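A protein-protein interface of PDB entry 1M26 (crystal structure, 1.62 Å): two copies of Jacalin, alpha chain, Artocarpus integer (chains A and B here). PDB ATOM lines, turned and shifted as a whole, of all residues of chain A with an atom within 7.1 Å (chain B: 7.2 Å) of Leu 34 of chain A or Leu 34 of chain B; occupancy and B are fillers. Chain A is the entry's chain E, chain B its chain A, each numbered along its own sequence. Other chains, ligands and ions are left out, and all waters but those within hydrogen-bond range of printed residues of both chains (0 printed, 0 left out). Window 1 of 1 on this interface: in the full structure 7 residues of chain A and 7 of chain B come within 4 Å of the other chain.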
ATOM      1  N   ASP A   6      16.910  24.820  14.905  1.00  0.00           N
ATOM      2  CA  ASP A   6      16.043  23.654  14.747  1.00  0.00           C
ATOM      3  C   ASP A   6      14.606  23.889  15.188  1.00  0.00           C
ATOM      4  O   ASP A   6      13.688  23.250  14.670  1.00  0.00           O
ATOM      5  CB  ASP A   6      16.581  22.453  15.523  1.00  0.00           C
ATOM      6  CG  ASP A   6      17.853  21.884  14.931  1.00  0.00           C
ATOM      7  OD1 ASP A   6      18.170  22.159  13.753  1.00  0.00           O
ATOM      8  OD2 ASP A   6      18.529  21.135  15.657  1.00  0.00           O
ATOM      9  N   GLY A   7      14.400  24.803  16.130  1.00  0.00           N
ATOM     10  CA  GLY A   7      13.057  25.038  16.620  1.00  0.00           C
ATOM     11  C   GLY A   7      12.783  24.145  17.823  1.00  0.00           C
ATOM     12  O   GLY A   7      13.706  23.531  18.365  1.00  0.00           O
ATOM     13  N   ALA A   8      11.523  24.064  18.242  1.00  0.00           N
ATOM     14  CA  ALA A   8      11.152  23.262  19.407  1.00  0.00           C
ATOM     15  C   ALA A   8      10.415  21.971  19.070  1.00  0.00           C
ATOM     16  O   ALA A   8       9.592  21.926  18.148  1.00  0.00           O
ATOM     17  CB  ALA A   8      10.301  24.098  20.353  1.00  0.00           C
ATOM     18  N   PHE A   9      10.699  20.929  19.847  1.00  0.00           N
ATOM     19  CA  PHE A   9      10.076  19.631  19.651  1.00  0.00           C
ATOM     20  C   PHE A   9       9.506  19.079  20.960  1.00  0.00           C
ATOM     21  O   PHE A   9       9.266  19.837  21.898  1.00  0.00           O
ATOM     22  CB  PHE A   9      11.086  18.665  19.028  1.00  0.00           C
ATOM     23  CG  PHE A   9      11.568  19.101  17.675  1.00  0.00           C
ATOM     24  CD1 PHE A   9      12.542  20.086  17.554  1.00  0.00           C
ATOM     25  CD2 PHE A   9      11.004  18.568  16.523  1.00  0.00           C
ATOM     26  CE1 PHE A   9      12.943  20.538  16.299  1.00  0.00           C
ATOM     27  CE2 PHE A   9      11.395  19.011  15.264  1.00  0.00           C
ATOM     28  CZ  PHE A   9      12.366  20.000  15.151  1.00  0.00           C
ATOM     29  N   THR A  10       9.283  17.768  21.021  1.00  0.00           N
ATOM     30  CA  THR A  10       8.708  17.125  22.212  1.00  0.00           C
ATOM     31  C   THR A  10       9.769  16.601  23.173  1.00  0.00           C
ATOM     32  O   THR A  10       9.482  16.346  24.343  1.00  0.00           O
ATOM     33  CB  THR A  10       7.773  15.897  22.069  1.00  0.00           C
ATOM     34  OG1 THR A  10       8.081  15.180  20.874  1.00  0.00           O
ATOM     35  CG2 THR A  10       6.321  16.352  22.012  1.00  0.00           C
ATOM     36  N   GLY A  11      10.979  16.410  22.667  1.00  0.00           N
ATOM     37  CA  GLY A  11      12.049  15.893  23.493  1.00  0.00           C
ATOM     38  C   GLY A  11      13.262  15.571  22.648  1.00  0.00           C
ATOM     39  O   GLY A  11      13.310  15.896  21.459  1.00  0.00           O
ATOM     40  N   ARG A  13      16.020  12.499  21.480  1.00  0.00           N
ATOM     41  CA  ARG A  13      16.248  11.068  21.441  1.00  0.00           C
ATOM     42  C   ARG A  13      17.715  10.710  21.266  1.00  0.00           C
ATOM     43  O   ARG A  13      18.188   9.725  21.826  1.00  0.00           O
ATOM     44  CB  ARG A  13      15.423  10.438  20.321  1.00  0.00           C
ATOM     45  CG  ARG A  13      13.972  10.230  20.723  1.00  0.00           C
ATOM     46  CD  ARG A  13      13.211   9.873  19.493  1.00  0.00           C
ATOM     47  NE  ARG A  13      11.798   9.578  19.684  1.00  0.00           N
ATOM     48  CZ  ARG A  13      11.313   8.394  20.039  1.00  0.00           C
ATOM     49  NH1 ARG A  13      12.114   7.367  20.285  1.00  0.00           N
ATOM     50  NH2 ARG A  13      10.006   8.197  20.016  1.00  0.00           N
ATOM     51  N   TYR A  32      15.293  14.425  17.383  1.00  0.00           N
ATOM     52  CA  TYR A  32      14.311  14.801  18.384  1.00  0.00           C
ATOM     53  C   TYR A  32      13.176  13.813  18.449  1.00  0.00           C
ATOM     54  O   TYR A  32      13.070  12.901  17.628  1.00  0.00           O
ATOM     55  CB  TYR A  32      13.689  16.157  18.045  1.00  0.00           C
ATOM     56  CG  TYR A  32      14.662  17.299  18.005  1.00  0.00           C
ATOM     57  CD1 TYR A  32      15.299  17.668  16.814  1.00  0.00           C
ATOM     58  CD2 TYR A  32      14.962  18.009  19.161  1.00  0.00           C
ATOM     59  CE1 TYR A  32      16.212  18.725  16.790  1.00  0.00           C
ATOM     60  CE2 TYR A  32      15.867  19.057  19.148  1.00  0.00           C
ATOM     61  CZ  TYR A  32      16.485  19.412  17.971  1.00  0.00           C
ATOM     62  OH  TYR A  32      17.369  20.461  17.988  1.00  0.00           O
ATOM     63  N   ASP A  33      12.343  13.989  19.462  1.00  0.00           N
ATOM     64  CA  ASP A  33      11.140  13.203  19.541  1.00  0.00           C
ATOM     65  C   ASP A  33      10.114  14.223  19.091  1.00  0.00           C
ATOM     66  O   ASP A  33      10.212  15.402  19.436  1.00  0.00           O
ATOM     67  CB  ASP A  33      10.768  12.780  20.955  1.00  0.00           C
ATOM     68  CG  ASP A  33       9.439  12.049  20.982  1.00  0.00           C
ATOM     69  OD1 ASP A  33       9.401  10.902  20.495  1.00  0.00           O
ATOM     70  OD2 ASP A  33       8.428  12.627  21.446  1.00  0.00           O
ATOM     71  N   LEU A  34       9.158  13.782  18.293  1.00  0.00           N
ATOM     72  CA  LEU A  34       8.099  14.666  17.847  1.00  0.00           C
ATOM     73  C   LEU A  34       6.807  13.905  18.055  1.00  0.00           C
ATOM     74  O   LEU A  34       6.406  13.110  17.207  1.00  0.00           O
ATOM     75  CB  LEU A  34       8.260  15.036  16.373  1.00  0.00           C
ATOM     76  CG  LEU A  34       7.121  15.925  15.845  1.00  0.00           C
ATOM     77  CD1 LEU A  34       7.075  17.237  16.627  1.00  0.00           C
ATOM     78  CD2 LEU A  34       7.323  16.195  14.360  1.00  0.00           C
ATOM     79  N   ASN A  35       6.175  14.141  19.203  1.00  0.00           N
ATOM     80  CA  ASN A  35       4.913  13.495  19.537  1.00  0.00           C
ATOM     81  C   ASN A  35       4.988  11.971  19.502  1.00  0.00           C
ATOM     82  O   ASN A  35       4.106  11.303  18.963  1.00  0.00           O
ATOM     83  CB  ASN A  35       3.821  14.005  18.593  1.00  0.00           C
ATOM     84  CG  ASN A  35       3.665  15.509  18.665  1.00  0.00           C
ATOM     85  OD1 ASN A  35       3.601  16.193  17.639  1.00  0.00           O
ATOM     86  ND2 ASN A  35       3.603  16.034  19.878  1.00  0.00           N
ATOM     87  N   GLY A  36       6.060  11.429  20.074  1.00  0.00           N
ATOM     88  CA  GLY A  36       6.222   9.985  20.133  1.00  0.00           C
ATOM     89  C   GLY A  36       6.957   9.313  18.992  1.00  0.00           C
ATOM     90  O   GLY A  36       7.159   8.099  19.013  1.00  0.00           O
ATOM     91  N   SER A  37       7.352  10.077  17.986  1.00  0.00           N
ATOM     92  CA  SER A  37       8.075   9.513  16.854  1.00  0.00           C
ATOM     93  C   SER A  37       9.387  10.263  16.644  1.00  0.00           C
ATOM     94  O   SER A  37       9.482  11.455  16.932  1.00  0.00           O
ATOM     95  CB  SER A  37       7.221   9.599  15.591  1.00  0.00           C
ATOM     96  OG  SER A  37       6.008   8.885  15.770  1.00  0.00           O
ATOM     97  N   PRO A  38      10.419   9.572  16.140  1.00  0.00           N
ATOM     98  CA  PRO A  38      11.706  10.232  15.913  1.00  0.00           C
ATOM     99  C   PRO A  38      11.634  11.244  14.779  1.00  0.00           C
ATOM    100  O   PRO A  38      10.942  11.030  13.780  1.00  0.00           O
ATOM    101  CB  PRO A  38      12.641   9.079  15.543  1.00  0.00           C
ATOM    102  CG  PRO A  38      11.935   7.845  16.033  1.00  0.00           C
ATOM    103  CD  PRO A  38      10.492   8.147  15.783  1.00  0.00           C
ATOM    104  N   TYR A  39      12.344  12.353  14.945  1.00  0.00           N
ATOM    105  CA  TYR A  39      12.423  13.371  13.908  1.00  0.00           C
ATOM    106  C   TYR A  39      13.906  13.669  13.764  1.00  0.00           C
ATOM    107  O   TYR A  39      14.546  14.178  14.687  1.00  0.00           O
ATOM    108  CB  TYR A  39      11.653  14.634  14.289  1.00  0.00           C
ATOM    109  CG  TYR A  39      11.782  15.736  13.260  1.00  0.00           C
ATOM    110  CD1 TYR A  39      12.858  16.622  13.291  1.00  0.00           C
ATOM    111  CD2 TYR A  39      10.858  15.859  12.225  1.00  0.00           C
ATOM    112  CE1 TYR A  39      13.015  17.601  12.313  1.00  0.00           C
ATOM    113  CE2 TYR A  39      11.009  16.837  11.240  1.00  0.00           C
ATOM    114  CZ  TYR A  39      12.092  17.702  11.293  1.00  0.00           C
ATOM    115  OH  TYR A  39      12.272  18.654  10.314  1.00  0.00           O
ATOM    116  N   PHE A  60      15.164   7.455  25.547  1.00  0.00           N
ATOM    117  CA  PHE A  60      14.043   8.369  25.568  1.00  0.00           C
ATOM    118  C   PHE A  60      12.775   7.625  26.002  1.00  0.00           C
ATOM    119  O   PHE A  60      12.602   6.459  25.567  1.00  0.00           O
ATOM    120  CB  PHE A  60      13.727   8.938  24.172  1.00  0.00           C
ATOM    121  CG  PHE A  60      12.499   9.815  24.149  1.00  0.00           C
ATOM    122  CD1 PHE A  60      12.562  11.100  24.682  1.00  0.00           C
ATOM    123  CD2 PHE A  60      11.302   9.356  23.631  1.00  0.00           C
ATOM    124  CE1 PHE A  60      11.437  11.926  24.683  1.00  0.00           C
ATOM    125  CE2 PHE A  60      10.165  10.170  23.625  1.00  0.00           C
ATOM    126  CZ  PHE A  60      10.235  11.460  24.148  1.00  0.00           C
ATOM    127  N   ASP B   6      -2.615  13.665  16.914  1.00  0.00           N
ATOM    128  CA  ASP B   6      -1.549  14.268  16.127  1.00  0.00           C
ATOM    129  C   ASP B   6      -0.413  14.804  16.989  1.00  0.00           C
ATOM    130  O   ASP B   6       0.743  14.805  16.570  1.00  0.00           O
ATOM    131  CB  ASP B   6      -2.090  15.411  15.261  1.00  0.00           C
ATOM    132  CG  ASP B   6      -2.951  14.925  14.106  1.00  0.00           C
ATOM    133  OD1 ASP B   6      -2.840  13.736  13.723  1.00  0.00           O
ATOM    134  OD2 ASP B   6      -3.724  15.751  13.575  1.00  0.00           O
ATOM    135  N   GLY B   7      -0.749  15.254  18.191  1.00  0.00           N
ATOM    136  CA  GLY B   7       0.255  15.814  19.080  1.00  0.00           C
ATOM    137  C   GLY B   7       0.292  17.323  18.933  1.00  0.00           C
ATOM    138  O   GLY B   7      -0.602  17.924  18.313  1.00  0.00           O
ATOM    139  N   ALA B   8       1.335  17.942  19.485  1.00  0.00           N
ATOM    140  CA  ALA B   8       1.478  19.396  19.441  1.00  0.00           C
ATOM    141  C   ALA B   8       2.496  19.864  18.420  1.00  0.00           C
ATOM    142  O   ALA B   8       3.541  19.233  18.215  1.00  0.00           O
ATOM    143  CB  ALA B   8       1.854  19.931  20.833  1.00  0.00           C
ATOM    144  N   PHE B   9       2.188  20.987  17.783  1.00  0.00           N
ATOM    145  CA  PHE B   9       3.070  21.556  16.778  1.00  0.00           C
ATOM    146  C   PHE B   9       3.289  23.039  17.034  1.00  0.00           C
ATOM    147  O   PHE B   9       3.039  23.517  18.144  1.00  0.00           O
ATOM    148  CB  PHE B   9       2.483  21.308  15.386  1.00  0.00           C
ATOM    149  CG  PHE B   9       2.413  19.850  15.023  1.00  0.00           C
ATOM    150  CD1 PHE B   9       1.401  19.035  15.532  1.00  0.00           C
ATOM    151  CD2 PHE B   9       3.405  19.277  14.235  1.00  0.00           C
ATOM    152  CE1 PHE B   9       1.385  17.662  15.261  1.00  0.00           C
ATOM    153  CE2 PHE B   9       3.401  17.913  13.961  1.00  0.00           C
ATOM    154  CZ  PHE B   9       2.390  17.103  14.478  1.00  0.00           C
ATOM    155  N   THR B  10       3.761  23.763  16.018  1.00  0.00           N
ATOM    156  CA  THR B  10       4.039  25.195  16.138  1.00  0.00           C
ATOM    157  C   THR B  10       2.865  26.075  15.742  1.00  0.00           C
ATOM    158  O   THR B  10       2.796  27.242  16.125  1.00  0.00           O
ATOM    159  CB  THR B  10       5.222  25.610  15.231  1.00  0.00           C
ATOM    160  OG1 THR B  10       6.269  24.643  15.333  1.00  0.00           O
ATOM    161  CG2 THR B  10       5.756  26.971  15.643  1.00  0.00           C
ATOM    162  N   GLY B  11       1.951  25.527  14.950  1.00  0.00           N
ATOM    163  CA  GLY B  11       0.815  26.311  14.511  1.00  0.00           C
ATOM    164  C   GLY B  11       0.016  25.511  13.509  1.00  0.00           C
ATOM    165  O   GLY B  11       0.309  24.337  13.269  1.00  0.00           O
ATOM    166  N   ARG B  13      -1.669  25.514   9.564  1.00  0.00           N
ATOM    167  CA  ARG B  13      -1.617  26.104   8.243  1.00  0.00           C
ATOM    168  C   ARG B  13      -2.866  25.859   7.419  1.00  0.00           C
ATOM    169  O   ARG B  13      -3.351  26.757   6.736  1.00  0.00           O
ATOM    170  CB  ARG B  13      -0.380  25.581   7.515  1.00  0.00           C
ATOM    171  CG  ARG B  13       0.939  26.179   8.023  1.00  0.00           C
ATOM    172  CD  ARG B  13       2.143  25.538   7.349  1.00  0.00           C
ATOM    173  NE  ARG B  13       3.409  26.212   7.639  1.00  0.00           N
ATOM    174  CZ  ARG B  13       4.001  27.123   6.879  1.00  0.00           C
ATOM    175  NH1 ARG B  13       5.162  27.665   7.256  1.00  0.00           N
ATOM    176  NH2 ARG B  13       3.421  27.481   5.771  1.00  0.00           N
ATOM    177  N   TYR B  32      -0.041  21.170   9.733  1.00  0.00           N
ATOM    178  CA  TYR B  32       0.448  22.016  10.800  1.00  0.00           C
ATOM    179  C   TYR B  32       1.693  22.747  10.352  1.00  0.00           C
ATOM    180  O   TYR B  32       2.178  22.566   9.237  1.00  0.00           O
ATOM    181  CB  TYR B  32       0.842  21.182  12.019  1.00  0.00           C
ATOM    182  CG  TYR B  32      -0.278  20.387  12.645  1.00  0.00           C
ATOM    183  CD1 TYR B  32      -0.512  19.058  12.282  1.00  0.00           C
ATOM    184  CD2 TYR B  32      -1.109  20.969  13.605  1.00  0.00           C
ATOM    185  CE1 TYR B  32      -1.549  18.329  12.861  1.00  0.00           C
ATOM    186  CE2 TYR B  32      -2.142  20.259  14.188  1.00  0.00           C
ATOM    187  CZ  TYR B  32      -2.363  18.942  13.817  1.00  0.00           C
ATOM    188  OH  TYR B  32      -3.398  18.261  14.418  1.00  0.00           O
ATOM    189  N   ASP B  33       2.190  23.611  11.225  1.00  0.00           N
ATOM    190  CA  ASP B  33       3.451  24.262  10.952  1.00  0.00           C
ATOM    191  C   ASP B  33       4.364  23.596  11.953  1.00  0.00           C
ATOM    192  O   ASP B  33       3.958  23.342  13.094  1.00  0.00           O
ATOM    193  CB  ASP B  33       3.452  25.757  11.257  1.00  0.00           C
ATOM    194  CG  ASP B  33       4.823  26.369  11.032  1.00  0.00           C
ATOM    195  OD1 ASP B  33       5.248  26.438   9.864  1.00  0.00           O
ATOM    196  OD2 ASP B  33       5.491  26.747  12.018  1.00  0.00           O
ATOM    197  N   LEU B  34       5.576  23.267  11.525  1.00  0.00           N
ATOM    198  CA  LEU B  34       6.551  22.669  12.425  1.00  0.00           C
ATOM    199  C   LEU B  34       7.823  23.489  12.290  1.00  0.00           C
ATOM    200  O   LEU B  34       8.647  23.247  11.411  1.00  0.00           O
ATOM    201  CB  LEU B  34       6.833  21.209  12.070  1.00  0.00           C
ATOM    202  CG  LEU B  34       7.912  20.571  12.960  1.00  0.00           C
ATOM    203  CD1 LEU B  34       7.425  20.505  14.401  1.00  0.00           C
ATOM    204  CD2 LEU B  34       8.248  19.182  12.449  1.00  0.00           C
ATOM    205  N   ASN B  35       7.956  24.483  13.157  1.00  0.00           N
ATOM    206  CA  ASN B  35       9.117  25.355  13.150  1.00  0.00           C
ATOM    207  C   ASN B  35       9.390  25.981  11.779  1.00  0.00           C
ATOM    208  O   ASN B  35      10.533  26.041  11.323  1.00  0.00           O
ATOM    209  CB  ASN B  35      10.336  24.579  13.659  1.00  0.00           C
ATOM    210  CG  ASN B  35      10.116  24.026  15.053  1.00  0.00           C
ATOM    211  OD1 ASN B  35      10.293  22.827  15.304  1.00  0.00           O
ATOM    212  ND2 ASN B  35       9.722  24.896  15.971  1.00  0.00           N
ATOM    213  N   GLY B  36       8.327  26.438  11.124  1.00  0.00           N
ATOM    214  CA  GLY B  36       8.479  27.095   9.842  1.00  0.00           C
ATOM    215  C   GLY B  36       8.249  26.248   8.613  1.00  0.00           C
ATOM    216  O   GLY B  36       8.196  26.775   7.505  1.00  0.00           O
ATOM    217  N   SER B  37       8.114  24.941   8.790  1.00  0.00           N
ATOM    218  CA  SER B  37       7.893  24.061   7.656  1.00  0.00           C
ATOM    219  C   SER B  37       6.527  23.407   7.737  1.00  0.00           C
ATOM    220  O   SER B  37       6.075  23.024   8.816  1.00  0.00           O
ATOM    221  CB  SER B  37       8.956  22.963   7.611  1.00  0.00           C
ATOM    222  OG  SER B  37      10.256  23.505   7.454  1.00  0.00           O
ATOM    223  N   PRO B  38       5.844  23.277   6.596  1.00  0.00           N
ATOM    224  CA  PRO B  38       4.529  22.637   6.640  1.00  0.00           C
ATOM    225  C   PRO B  38       4.710  21.180   7.056  1.00  0.00           C
ATOM    226  O   PRO B  38       5.604  20.496   6.561  1.00  0.00           O
ATOM    227  CB  PRO B  38       4.040  22.732   5.193  1.00  0.00           C
ATOM    228  CG  PRO B  38       4.803  23.907   4.631  1.00  0.00           C
ATOM    229  CD  PRO B  38       6.165  23.754   5.239  1.00  0.00           C
ATOM    230  N   TYR B  39       3.873  20.714   7.970  1.00  0.00           N
ATOM    231  CA  TYR B  39       3.918  19.330   8.400  1.00  0.00           C
ATOM    232  C   TYR B  39       2.585  18.719   7.971  1.00  0.00           C
ATOM    233  O   TYR B  39       1.522  19.081   8.479  1.00  0.00           O
ATOM    234  CB  TYR B  39       4.097  19.246   9.920  1.00  0.00           C
ATOM    235  CG  TYR B  39       4.135  17.833  10.450  1.00  0.00           C
ATOM    236  CD1 TYR B  39       2.961  17.104  10.621  1.00  0.00           C
ATOM    237  CD2 TYR B  39       5.349  17.219  10.774  1.00  0.00           C
ATOM    238  CE1 TYR B  39       2.985  15.804  11.100  1.00  0.00           C
ATOM    239  CE2 TYR B  39       5.383  15.914  11.255  1.00  0.00           C
ATOM    240  CZ  TYR B  39       4.198  15.216  11.414  1.00  0.00           C
ATOM    241  OH  TYR B  39       4.221  13.922  11.885  1.00  0.00           O
ATOM    242  N   PHE B  60      -1.381  31.581   7.345  1.00  0.00           N
ATOM    243  CA  PHE B  60      -0.444  31.382   8.449  1.00  0.00           C
ATOM    244  C   PHE B  60       0.588  32.419   8.053  1.00  0.00           C
ATOM    245  O   PHE B  60       1.124  32.625   6.968  1.00  0.00           O
ATOM    246  CB  PHE B  60       0.214  30.009   8.360  1.00  0.00           C
ATOM    247  CG  PHE B  60       1.219  29.752   9.445  1.00  0.00           C
ATOM    248  CD1 PHE B  60       0.789  29.568  10.750  1.00  0.00           C
ATOM    249  CD2 PHE B  60       2.588  29.713   9.176  1.00  0.00           C
ATOM    250  CE1 PHE B  60       1.691  29.348  11.774  1.00  0.00           C
ATOM    251  CE2 PHE B  60       3.507  29.492  10.205  1.00  0.00           C
ATOM    252  CZ  PHE B  60       3.055  29.308  11.504  1.00  0.00           C
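N of Ala 8 of chain B lies close to ND2 of Asn 35 of chain A, 3.0 Å away. The side-chain amide oxygen of Asn 35 of chain B sits close to the backbone carbonyl oxygen of Asp 6 of chain A (3.5 Å). The side-chain amide nitrogen (ND2) of Asn 35 of chain B lies close to the backbone NH (N) of Ala 8 of chain A, 3.0 Å away. The backbone carbonyl oxygen (O) of Asp 6 of chain B sits close to the side-chain amide oxygen (OD1) of Asn 35 of chain A, 3.4 Å away.
N of Tyr 39 of chain B lies within hydrogen-bond range of O of Tyr 32 of chain B (2.8 Å). OD2 of Asp 6 of chain A lies within hydrogen-bond range of OH of Tyr 32 of chain A (2.7 Å). The backbone carbonyl oxygen (O) of Tyr 39 of chain A sits at hydrogen-bond distance from the backbone NH (N) of Tyr 32 of chain A (2.8 Å). N of Asn 35 of chain A sits at hydrogen-bond distance from OG1 of Thr 10 of chain A (2.7 Å). The side-chain carboxylate of Asp 6 of chain B is in hydrogen-bond range of the side-chain hydroxyl of Tyr 32 of chain B, 2.7 Å away. OG1 of Thr 10 of chain B is in hydrogen-bond range of N of Asn 35 of chain B (2.8 Å).
Asn 35 of chain B touches Gly 7 of chain A (ND2 to CA, 3.4 Å). CZ of Phe 9 of chain A touches OD1 of Asn 35 of chain B, 3.5 Å away. Leu 34 of chain A touches Leu 34 of chain B (CD2 to CD2, 3.7 Å). Leu 34 of chain A touches Tyr 39 of chain B (CD2 to CE2, 3.7 Å). CA of Gly 7 of chain B touches CG of Asn 35 of chain A, 3.4 Å away. Phe 9 of chain B touches Asn 35 of chain A (CZ to OD1, 3.5 Å). Tyr 39 of chain A touches Leu 34 of chain B.
Of the printed residues of chain B, Ala 8 of chain A touches Asn 35 (3.0 Å). Printed residues of chain B within 4 Å of Phe 9 of chain A: Asn 35. Leu 34 of chain A touches just these residues of chain B: Leu 34 (3.7 Å) and Tyr 39 (3.7 Å). Of the printed residues of chain B, Tyr 39 of chain A touches Leu 34. Thr 10 of chain B touches none of the printed residues of chain A. Gly 11 of chain B touches none of the printed residues of chain A. Leu 34 of chain B touches just these residues of chain A: Leu 34 and Tyr 39. Of the printed residues of chain A, Asn 35 of chain B touches Asp 6, Gly 7, Ala 8 and Phe 9.
Printed residues of chain A that touch a printed residue of chain B: Asp 6, Gly 7, Ala 8, Phe 9, Leu 34, Asn 35 and Tyr 39. Among the printed residues, 11 pairs touch across the chains. Among the printed residues, no Asp or Glu carboxylate lies within 4 Å of a Lys or Arg side-chain nitrogen of the other chain.
Asp 6 of chain A touches Asn 35 of chain B, and with the chains exchanged Asn 35 of chain A touches Asp 6 of chain B. Gly 7 of chain A touches Asn 35 of chain B, and with the chains exchanged Asn 35 of chain A touches Gly 7 of chain B. Ala 8 of chain A touches Asn 35 of chain B, and with the chains exchanged Asn 35 of chain A touches Ala 8 of chain B. Phe 9 of chain A touches Asn 35 of chain B, and with the chains exchanged Asn 35 of chain A touches Phe 9 of chain B. Positions printed for both chains: 6, 7, 8, 9, 10, 11, 13, 32, 33, 34, 35, 36, 37, 38, 39 and 60.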
